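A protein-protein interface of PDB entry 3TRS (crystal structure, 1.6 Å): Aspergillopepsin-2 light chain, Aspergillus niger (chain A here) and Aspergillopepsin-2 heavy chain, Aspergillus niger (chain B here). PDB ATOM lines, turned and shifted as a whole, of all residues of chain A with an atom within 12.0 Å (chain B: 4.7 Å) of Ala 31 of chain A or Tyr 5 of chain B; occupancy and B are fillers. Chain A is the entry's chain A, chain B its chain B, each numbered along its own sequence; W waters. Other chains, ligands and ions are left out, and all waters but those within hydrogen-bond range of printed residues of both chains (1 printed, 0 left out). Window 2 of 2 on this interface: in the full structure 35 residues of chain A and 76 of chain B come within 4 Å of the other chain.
CZ of Phe 29 of chain B touches CD of Pro 27 of chain A, 3.8 Å away.
O of Ser 28 of chain A touches O of Asp 123 of chain B, 3.9 Å away.
Val 29 of chain A touches Phe 29 of chain B.
Cys 30 of chain B touches Val 29 of chain A (O to CG2, 3.5 Å).
O of Asp 123 of chain B touches CA of Val 29 of chain A, at 3.4 Å.
Ser 30 of chain A touches Tyr 31 of chain B.
Tyr 31 of chain B touches Ala 31 of chain A (CD2 to N, 3.4 Å).
Asp 123 of chain B touches Ala 31 of chain A.
N of Gly 32 of chain A touches CD2 of Tyr 5 of chain B, at 3.1 Å.
Gly 32 of chain A touches Asp 123 of chain B (N to N, 3.7 Å).
Hydrophobic or aromatic side chains of chain B that line the printed part of chain A: Tyr 5, Phe 29, Tyr 31 and Ala 122.
Of the 12 printed residues of chain A, 6 touch a printed residue of chain B.
Among the printed residues, 16 pairs touch across the chains.
Water W1 bridges O of Phe 121 of chain B and O of Ser 34 of chain A.
Of chain B, only Tyr 5 (3.5 Å), Tyr 31 (3.4 Å) and Asp 123 (3.3 Å) come within 4 Å of Ala 31 of chain A.
Of the printed residues of chain A, Tyr 5 of chain B touches Ala 31 and Gly 32.
No residue of chain A comes within 4 Å of Glu 3 of chain B.
No residue of chain A comes within 4 Å of Ala 7 of chain B.
Cys 30 of chain B touches just one residue of chain A: Val 29 (3.5 Å).
Of chain A, only Val 29 (3.4 Å), Ser 30 (3.7 Å) and Ala 31 (3.4 Å) come within 4 Å of Tyr 31 of chain B.
No residue of chain A comes within 4 Å of Val 119 of chain B.
No residue of chain A comes within 4 Å of Ala 120 of chain B.
Asp 123 of chain B touches five residues of chain A.
Printed residues of chain B within 4 Å of Pro 27 of chain A: Phe 29 (3.8 Å).
Printed residues of chain B within 4 Å of Val 29 of chain A: Phe 29, Cys 30, Tyr 31, Ala 122 and Asp 123.
Printed residues of chain B within 4 Å of Gly 32 of chain A: Tyr 5 (3.1 Å), Phe 121 (3.3 Å) and Asp 123 (3.7 Å).
The nearest printed residue of chain B that does not touch Ala 31 of chain A is Ala 122 of chain B (4.8 Å).
The nearest residue of chain A that does not touch Tyr 5 of chain B is Ser 30 of chain A (4.3 Å).
N of Ser 30 of chain A is in hydrogen-bond range of O of Asp 123 of chain B (2.8 Å).
OE1 of Glu 3 of chain B sits at hydrogen-bond distance from OH of Tyr 5 of chain B (2.8 Å).
The backbone carbonyl oxygen (O) of Ala 7 of chain B lies within hydrogen-bond range of the backbone NH (N) of Phe 29 of chain B (2.6 Å).
The backbone carbonyl oxygen (O) of Tyr 5 of chain B sits at hydrogen-bond distance from the backbone NH (N) of Tyr 31 of chain B, at 2.5 Å.
The backbone NH (N) of Ala 122 of chain B is in hydrogen-bond range of the backbone carbonyl oxygen (O) of Cys 6 of chain B, at 2.8 Å.
SG of Cys 6 of chain B forms a disulfide with SG of Cys 30 of chain B (2.0 Å).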
ATOM      1  N   VAL A  26     -25.473 -20.817  34.132  1.00  0.00           N
ATOM      2  CA  VAL A  26     -24.611 -20.647  33.001  1.00  0.00           C
ATOM      3  C   VAL A  26     -25.414 -19.922  31.937  1.00  0.00           C
ATOM      4  O   VAL A  26     -26.461 -20.388  31.500  1.00  0.00           O
ATOM      5  CB  VAL A  26     -24.114 -22.001  32.536  1.00  0.00           C
ATOM      6  CG1 VAL A  26     -23.265 -21.853  31.307  1.00  0.00           C
ATOM      7  CG2 VAL A  26     -23.306 -22.625  33.644  1.00  0.00           C
ATOM      8  N   PRO A  27     -24.942 -18.740  31.545  1.00  0.00           N
ATOM      9  CA  PRO A  27     -25.766 -18.006  30.623  1.00  0.00           C
ATOM     10  C   PRO A  27     -25.439 -18.445  29.205  1.00  0.00           C
ATOM     11  O   PRO A  27     -24.426 -19.116  28.970  1.00  0.00           O
ATOM     12  CB  PRO A  27     -25.350 -16.552  30.871  1.00  0.00           C
ATOM     13  CG  PRO A  27     -23.893 -16.655  31.282  1.00  0.00           C
ATOM     14  CD  PRO A  27     -23.674 -18.055  31.841  1.00  0.00           C
ATOM     15  N   SER A  28     -26.325 -18.112  28.286  1.00  0.00           N
ATOM     16  CA  SER A  28     -25.984 -18.197  26.885  1.00  0.00           C
ATOM     17  C   SER A  28     -24.900 -17.153  26.659  1.00  0.00           C
ATOM     18  O   SER A  28     -24.957 -16.053  27.226  1.00  0.00           O
ATOM     19  CB  SER A  28     -27.207 -17.928  26.008  1.00  0.00           C
ATOM     20  OG  SER A  28     -27.855 -16.749  26.409  1.00  0.00           O
ATOM     21  N   VAL A  29     -23.882 -17.527  25.898  1.00  0.00           N
ATOM     22  CA  VAL A  29     -22.880 -16.574  25.445  1.00  0.00           C
ATOM     23  C   VAL A  29     -23.083 -16.311  23.987  1.00  0.00           C
ATOM     24  O   VAL A  29     -23.482 -17.185  23.223  1.00  0.00           O
ATOM     25  CB  VAL A  29     -21.423 -17.042  25.600  1.00  0.00           C
ATOM     26  CG1 VAL A  29     -20.848 -16.514  26.860  1.00  0.00           C
ATOM     27  CG2 VAL A  29     -21.282 -18.553  25.473  1.00  0.00           C
ATOM     28  N   SER A  30     -22.815 -15.081  23.603  1.00  0.00           N
ATOM     29  CA  SER A  30     -22.782 -14.760  22.211  1.00  0.00           C
ATOM     30  C   SER A  30     -21.510 -13.983  21.991  1.00  0.00           C
ATOM     31  O   SER A  30     -20.756 -13.694  22.934  1.00  0.00           O
ATOM     32  CB  SER A  30     -24.020 -13.950  21.815  1.00  0.00           C
ATOM     33  OG  SER A  30     -24.352 -13.001  22.811  1.00  0.00           O
ATOM     34  N   ALA A  31     -21.254 -13.655  20.735  1.00  0.00           N
ATOM     35  CA  ALA A  31     -20.126 -12.815  20.428  1.00  0.00           C
ATOM     36  C   ALA A  31     -20.288 -11.501  21.170  1.00  0.00           C
ATOM     37  O   ALA A  31     -21.402 -11.024  21.374  1.00  0.00           O
ATOM     38  CB  ALA A  31     -20.048 -12.583  18.921  1.00  0.00           C
ATOM     39  N   GLY A  32     -19.175 -10.944  21.622  1.00  0.00           N
ATOM     40  CA  GLY A  32     -19.171  -9.609  22.199  1.00  0.00           C
ATOM     41  C   GLY A  32     -19.135  -8.553  21.116  1.00  0.00           C
ATOM     42  O   GLY A  32     -18.604  -8.787  20.041  1.00  0.00           O
ATOM     43  N   SER A  33     -19.725  -7.394  21.395  1.00  0.00           N
ATOM     44  CA  SER A  33     -19.788  -6.309  20.412  1.00  0.00           C
ATOM     45  C   SER A  33     -19.096  -5.067  20.956  1.00  0.00           C
ATOM     46  O   SER A  33     -18.822  -4.107  20.227  1.00  0.00           O
ATOM     47  CB  SER A  33     -21.231  -6.010  20.014  1.00  0.00           C
ATOM     48  OG  SER A  33     -21.582  -6.720  18.828  1.00  0.00           O
ATOM     49  N   SER A  34     -18.801  -5.106  22.247  1.00  0.00           N
ATOM     50  CA  SER A  34     -17.977  -4.095  22.864  1.00  0.00           C
ATOM     51  C   SER A  34     -16.551  -4.445  22.461  1.00  0.00           C
ATOM     52  O   SER A  34     -16.334  -5.340  21.621  1.00  0.00           O
ATOM     53  CB  SER A  34     -18.177  -4.104  24.376  1.00  0.00           C
ATOM     54  OG  SER A  34     -19.560  -4.078  24.692  1.00  0.00           O
ATOM     55  N   GLY A  35     -15.570  -3.748  23.012  1.00  0.00           N
ATOM     56  CA  GLY A  35     -14.201  -4.008  22.589  1.00  0.00           C
ATOM     57  C   GLY A  35     -13.848  -3.158  21.385  1.00  0.00           C
ATOM     58  O   GLY A  35     -14.717  -2.733  20.609  1.00  0.00           O
ATOM     59  N   SER A  36     -12.554  -2.932  21.223  1.00  0.00           N
ATOM     60  CA  SER A  36     -12.064  -1.900  20.336  1.00  0.00           C
ATOM     61  C   SER A  36     -11.835  -2.390  18.921  1.00  0.00           C
ATOM     62  O   SER A  36     -11.618  -3.577  18.673  1.00  0.00           O
ATOM     63  CB  SER A  36     -10.772  -1.307  20.896  1.00  0.00           C
ATOM     64  OG  SER A  36      -9.809  -2.325  21.130  1.00  0.00           O
ATOM     65  N   SER A  37     -11.891  -1.451  17.989  1.00  0.00           N
ATOM     66  CA  SER A  37     -11.465  -1.731  16.635  1.00  0.00           C
ATOM     67  C   SER A  37     -10.765  -0.522  16.048  1.00  0.00           C
ATOM     68  O   SER A  37     -11.140   0.627  16.318  1.00  0.00           O
ATOM     69  CB  SER A  37     -12.650  -2.117  15.759  1.00  0.00           C
ATOM     70  OG  SER A  37     -13.494  -1.005  15.563  1.00  0.00           O
ATOM     71  N   GLU B   3     -14.284 -15.096  15.541  1.00  0.00           N
ATOM     72  CA  GLU B   3     -13.218 -15.132  16.582  1.00  0.00           C
ATOM     73  C   GLU B   3     -13.822 -15.683  17.865  1.00  0.00           C
ATOM     74  O   GLU B   3     -15.047 -15.723  18.026  1.00  0.00           O
ATOM     75  CB  GLU B   3     -12.608 -13.737  16.782  1.00  0.00           C
ATOM     76  CG  GLU B   3     -13.226 -12.849  17.861  1.00  0.00           C
ATOM     77  CD  GLU B   3     -13.077 -11.353  17.580  1.00  0.00           C
ATOM     78  OE1 GLU B   3     -13.779 -10.834  16.689  1.00  0.00           O
ATOM     79  OE2 GLU B   3     -12.267 -10.682  18.267  1.00  0.00           O
ATOM     80  N   GLU B   4     -12.964 -16.099  18.778  1.00  0.00           N
ATOM     81  CA  GLU B   4     -13.457 -16.638  20.016  1.00  0.00           C
ATOM     82  C   GLU B   4     -13.764 -15.522  20.993  1.00  0.00           C
ATOM     83  O   GLU B   4     -12.967 -14.598  21.183  1.00  0.00           O
ATOM     84  CB  GLU B   4     -12.461 -17.611  20.616  1.00  0.00           C
ATOM     85  CG  GLU B   4     -12.975 -18.225  21.886  1.00  0.00           C
ATOM     86  CD  GLU B   4     -12.541 -19.641  22.065  1.00  0.00           C
ATOM     87  OE1 GLU B   4     -12.456 -20.370  21.049  1.00  0.00           O
ATOM     88  OE2 GLU B   4     -12.295 -20.022  23.227  1.00  0.00           O
ATOM     89  N   TYR B   5     -14.920 -15.623  21.625  1.00  0.00           N
ATOM     90  CA  TYR B   5     -15.239 -14.714  22.687  1.00  0.00           C
ATOM     91  C   TYR B   5     -15.487 -15.551  23.881  1.00  0.00           C
ATOM     92  O   TYR B   5     -16.193 -16.541  23.825  1.00  0.00           O
ATOM     93  CB  TYR B   5     -16.481 -13.902  22.423  1.00  0.00           C
ATOM     94  CG  TYR B   5     -16.416 -13.063  21.208  1.00  0.00           C
ATOM     95  CD1 TYR B   5     -16.603 -13.617  19.957  1.00  0.00           C
ATOM     96  CD2 TYR B   5     -16.205 -11.694  21.306  1.00  0.00           C
ATOM     97  CE1 TYR B   5     -16.584 -12.835  18.840  1.00  0.00           C
ATOM     98  CE2 TYR B   5     -16.168 -10.892  20.180  1.00  0.00           C
ATOM     99  CZ  TYR B   5     -16.369 -11.473  18.950  1.00  0.00           C
ATOM    100  OH  TYR B   5     -16.338 -10.714  17.815  1.00  0.00           O
ATOM    101  N   CYS B   6     -14.864 -15.168  24.955  1.00  0.00           N
ATOM    102  CA  CYS B   6     -15.084 -15.849  26.180  1.00  0.00           C
ATOM    103  C   CYS B   6     -15.206 -14.883  27.293  1.00  0.00           C
ATOM    104  O   CYS B   6     -14.893 -13.706  27.191  1.00  0.00           O
ATOM    105  CB  CYS B   6     -13.914 -16.755  26.505  1.00  0.00           C
ATOM    106  SG  CYS B   6     -13.497 -17.908  25.268  1.00  0.00           S
ATOM    107  N   ALA B   7     -15.680 -15.432  28.393  1.00  0.00           N
ATOM    108  CA  ALA B   7     -15.667 -14.768  29.661  1.00  0.00           C
ATOM    109  C   ALA B   7     -15.563 -15.924  30.595  1.00  0.00           C
ATOM    110  O   ALA B   7     -15.843 -17.060  30.222  1.00  0.00           O
ATOM    111  CB  ALA B   7     -16.960 -14.011  29.886  1.00  0.00           C
ATOM    112  N   PHE B  29     -17.000 -19.350  29.626  1.00  0.00           N
ATOM    113  CA  PHE B  29     -18.028 -19.425  28.602  1.00  0.00           C
ATOM    114  C   PHE B  29     -17.371 -18.904  27.355  1.00  0.00           C
ATOM    115  O   PHE B  29     -16.913 -17.771  27.324  1.00  0.00           O
ATOM    116  CB  PHE B  29     -19.217 -18.542  28.903  1.00  0.00           C
ATOM    117  CG  PHE B  29     -19.488 -18.315  30.352  1.00  0.00           C
ATOM    118  CD1 PHE B  29     -19.684 -19.372  31.222  1.00  0.00           C
ATOM    119  CD2 PHE B  29     -19.627 -17.014  30.823  1.00  0.00           C
ATOM    120  CE1 PHE B  29     -19.972 -19.139  32.556  1.00  0.00           C
ATOM    121  CE2 PHE B  29     -19.900 -16.781  32.153  1.00  0.00           C
ATOM    122  CZ  PHE B  29     -20.090 -17.836  33.011  1.00  0.00           C
ATOM    123  N   CYS B  30     -17.358 -19.707  26.307  1.00  0.00           N
ATOM    124  CA  CYS B  30     -16.783 -19.239  25.075  1.00  0.00           C
ATOM    125  C   CYS B  30     -17.771 -19.362  23.984  1.00  0.00           C
ATOM    126  O   CYS B  30     -18.632 -20.226  23.983  1.00  0.00           O
ATOM    127  CB  CYS B  30     -15.518 -19.984  24.725  1.00  0.00           C
ATOM    128  SG  CYS B  30     -14.286 -19.631  25.901  1.00  0.00           S
ATOM    129  N   TYR B  31     -17.632 -18.467  23.038  1.00  0.00           N
ATOM    130  CA  TYR B  31     -18.472 -18.509  21.892  1.00  0.00           C
ATOM    131  C   TYR B  31     -17.510 -18.300  20.781  1.00  0.00           C
ATOM    132  O   TYR B  31     -16.694 -17.403  20.839  1.00  0.00           O
ATOM    133  CB  TYR B  31     -19.459 -17.365  21.941  1.00  0.00           C
ATOM    134  CG  TYR B  31     -20.249 -17.231  20.677  1.00  0.00           C
ATOM    135  CD1 TYR B  31     -21.509 -17.799  20.568  1.00  0.00           C
ATOM    136  CD2 TYR B  31     -19.741 -16.518  19.587  1.00  0.00           C
ATOM    137  CE1 TYR B  31     -22.246 -17.679  19.406  1.00  0.00           C
ATOM    138  CE2 TYR B  31     -20.474 -16.392  18.422  1.00  0.00           C
ATOM    139  CZ  TYR B  31     -21.724 -16.976  18.342  1.00  0.00           C
ATOM    140  OH  TYR B  31     -22.463 -16.857  17.193  1.00  0.00           O
ATOM    141  N   VAL B 119      -8.825 -12.579  25.898  1.00  0.00           N
ATOM    142  CA  VAL B 119      -9.765 -13.140  24.967  1.00  0.00           C
ATOM    143  C   VAL B 119     -10.807 -12.091  24.710  1.00  0.00           C
ATOM    144  O   VAL B 119     -11.148 -11.317  25.598  1.00  0.00           O
ATOM    145  CB  VAL B 119     -10.383 -14.439  25.486  1.00  0.00           C
ATOM    146  CG1 VAL B 119     -11.338 -14.156  26.617  1.00  0.00           C
ATOM    147  CG2 VAL B 119     -11.071 -15.223  24.372  1.00  0.00           C
ATOM    148  N   ALA B 120     -11.272 -12.046  23.464  1.00  0.00           N
ATOM    149  CA  ALA B 120     -12.369 -11.197  23.110  1.00  0.00           C
ATOM    150  C   ALA B 120     -13.489 -11.505  24.056  1.00  0.00           C
ATOM    151  O   ALA B 120     -13.808 -12.657  24.310  1.00  0.00           O
ATOM    152  CB  ALA B 120     -12.784 -11.428  21.691  1.00  0.00           C
ATOM    153  N   PHE B 121     -14.070 -10.468  24.597  1.00  0.00           N
ATOM    154  CA  PHE B 121     -14.911 -10.664  25.753  1.00  0.00           C
ATOM    155  C   PHE B 121     -16.277 -11.053  25.292  1.00  0.00           C
ATOM    156  O   PHE B 121     -16.932 -10.290  24.596  1.00  0.00           O
ATOM    157  CB  PHE B 121     -14.996  -9.374  26.505  1.00  0.00           C
ATOM    158  CG  PHE B 121     -15.476  -9.532  27.894  1.00  0.00           C
ATOM    159  CD1 PHE B 121     -15.057 -10.604  28.666  1.00  0.00           C
ATOM    160  CD2 PHE B 121     -16.333  -8.601  28.435  1.00  0.00           C
ATOM    161  CE1 PHE B 121     -15.481 -10.737  29.965  1.00  0.00           C
ATOM    162  CE2 PHE B 121     -16.772  -8.745  29.751  1.00  0.00           C
ATOM    163  CZ  PHE B 121     -16.347  -9.793  30.503  1.00  0.00           C
ATOM    164  N   ALA B 122     -16.726 -12.239  25.695  1.00  0.00           N
ATOM    165  CA  ALA B 122     -18.008 -12.724  25.218  1.00  0.00           C
ATOM    166  C   ALA B 122     -19.112 -11.900  25.811  1.00  0.00           C
ATOM    167  O   ALA B 122     -19.030 -11.436  26.938  1.00  0.00           O
ATOM    168  CB  ALA B 122     -18.214 -14.178  25.580  1.00  0.00           C
ATOM    169  N   ASP B 123     -20.173 -11.761  25.045  1.00  0.00           N
ATOM    170  CA  ASP B 123     -21.375 -11.247  25.596  1.00  0.00           C
ATOM    171  C   ASP B 123     -22.064 -12.416  26.286  1.00  0.00           C
ATOM    172  O   ASP B 123     -22.742 -13.218  25.650  1.00  0.00           O
ATOM    173  CB  ASP B 123     -22.250 -10.681  24.498  1.00  0.00           C
ATOM    174  CG  ASP B 123     -23.566 -10.179  25.023  1.00  0.00           C
ATOM    175  OD1 ASP B 123     -23.824 -10.282  26.254  1.00  0.00           O
ATOM    176  OD2 ASP B 123     -24.335  -9.657  24.195  1.00  0.00           O
HETATM  177  O   HOH W   1     -16.858  -7.913  23.861  1.00  0.00           O
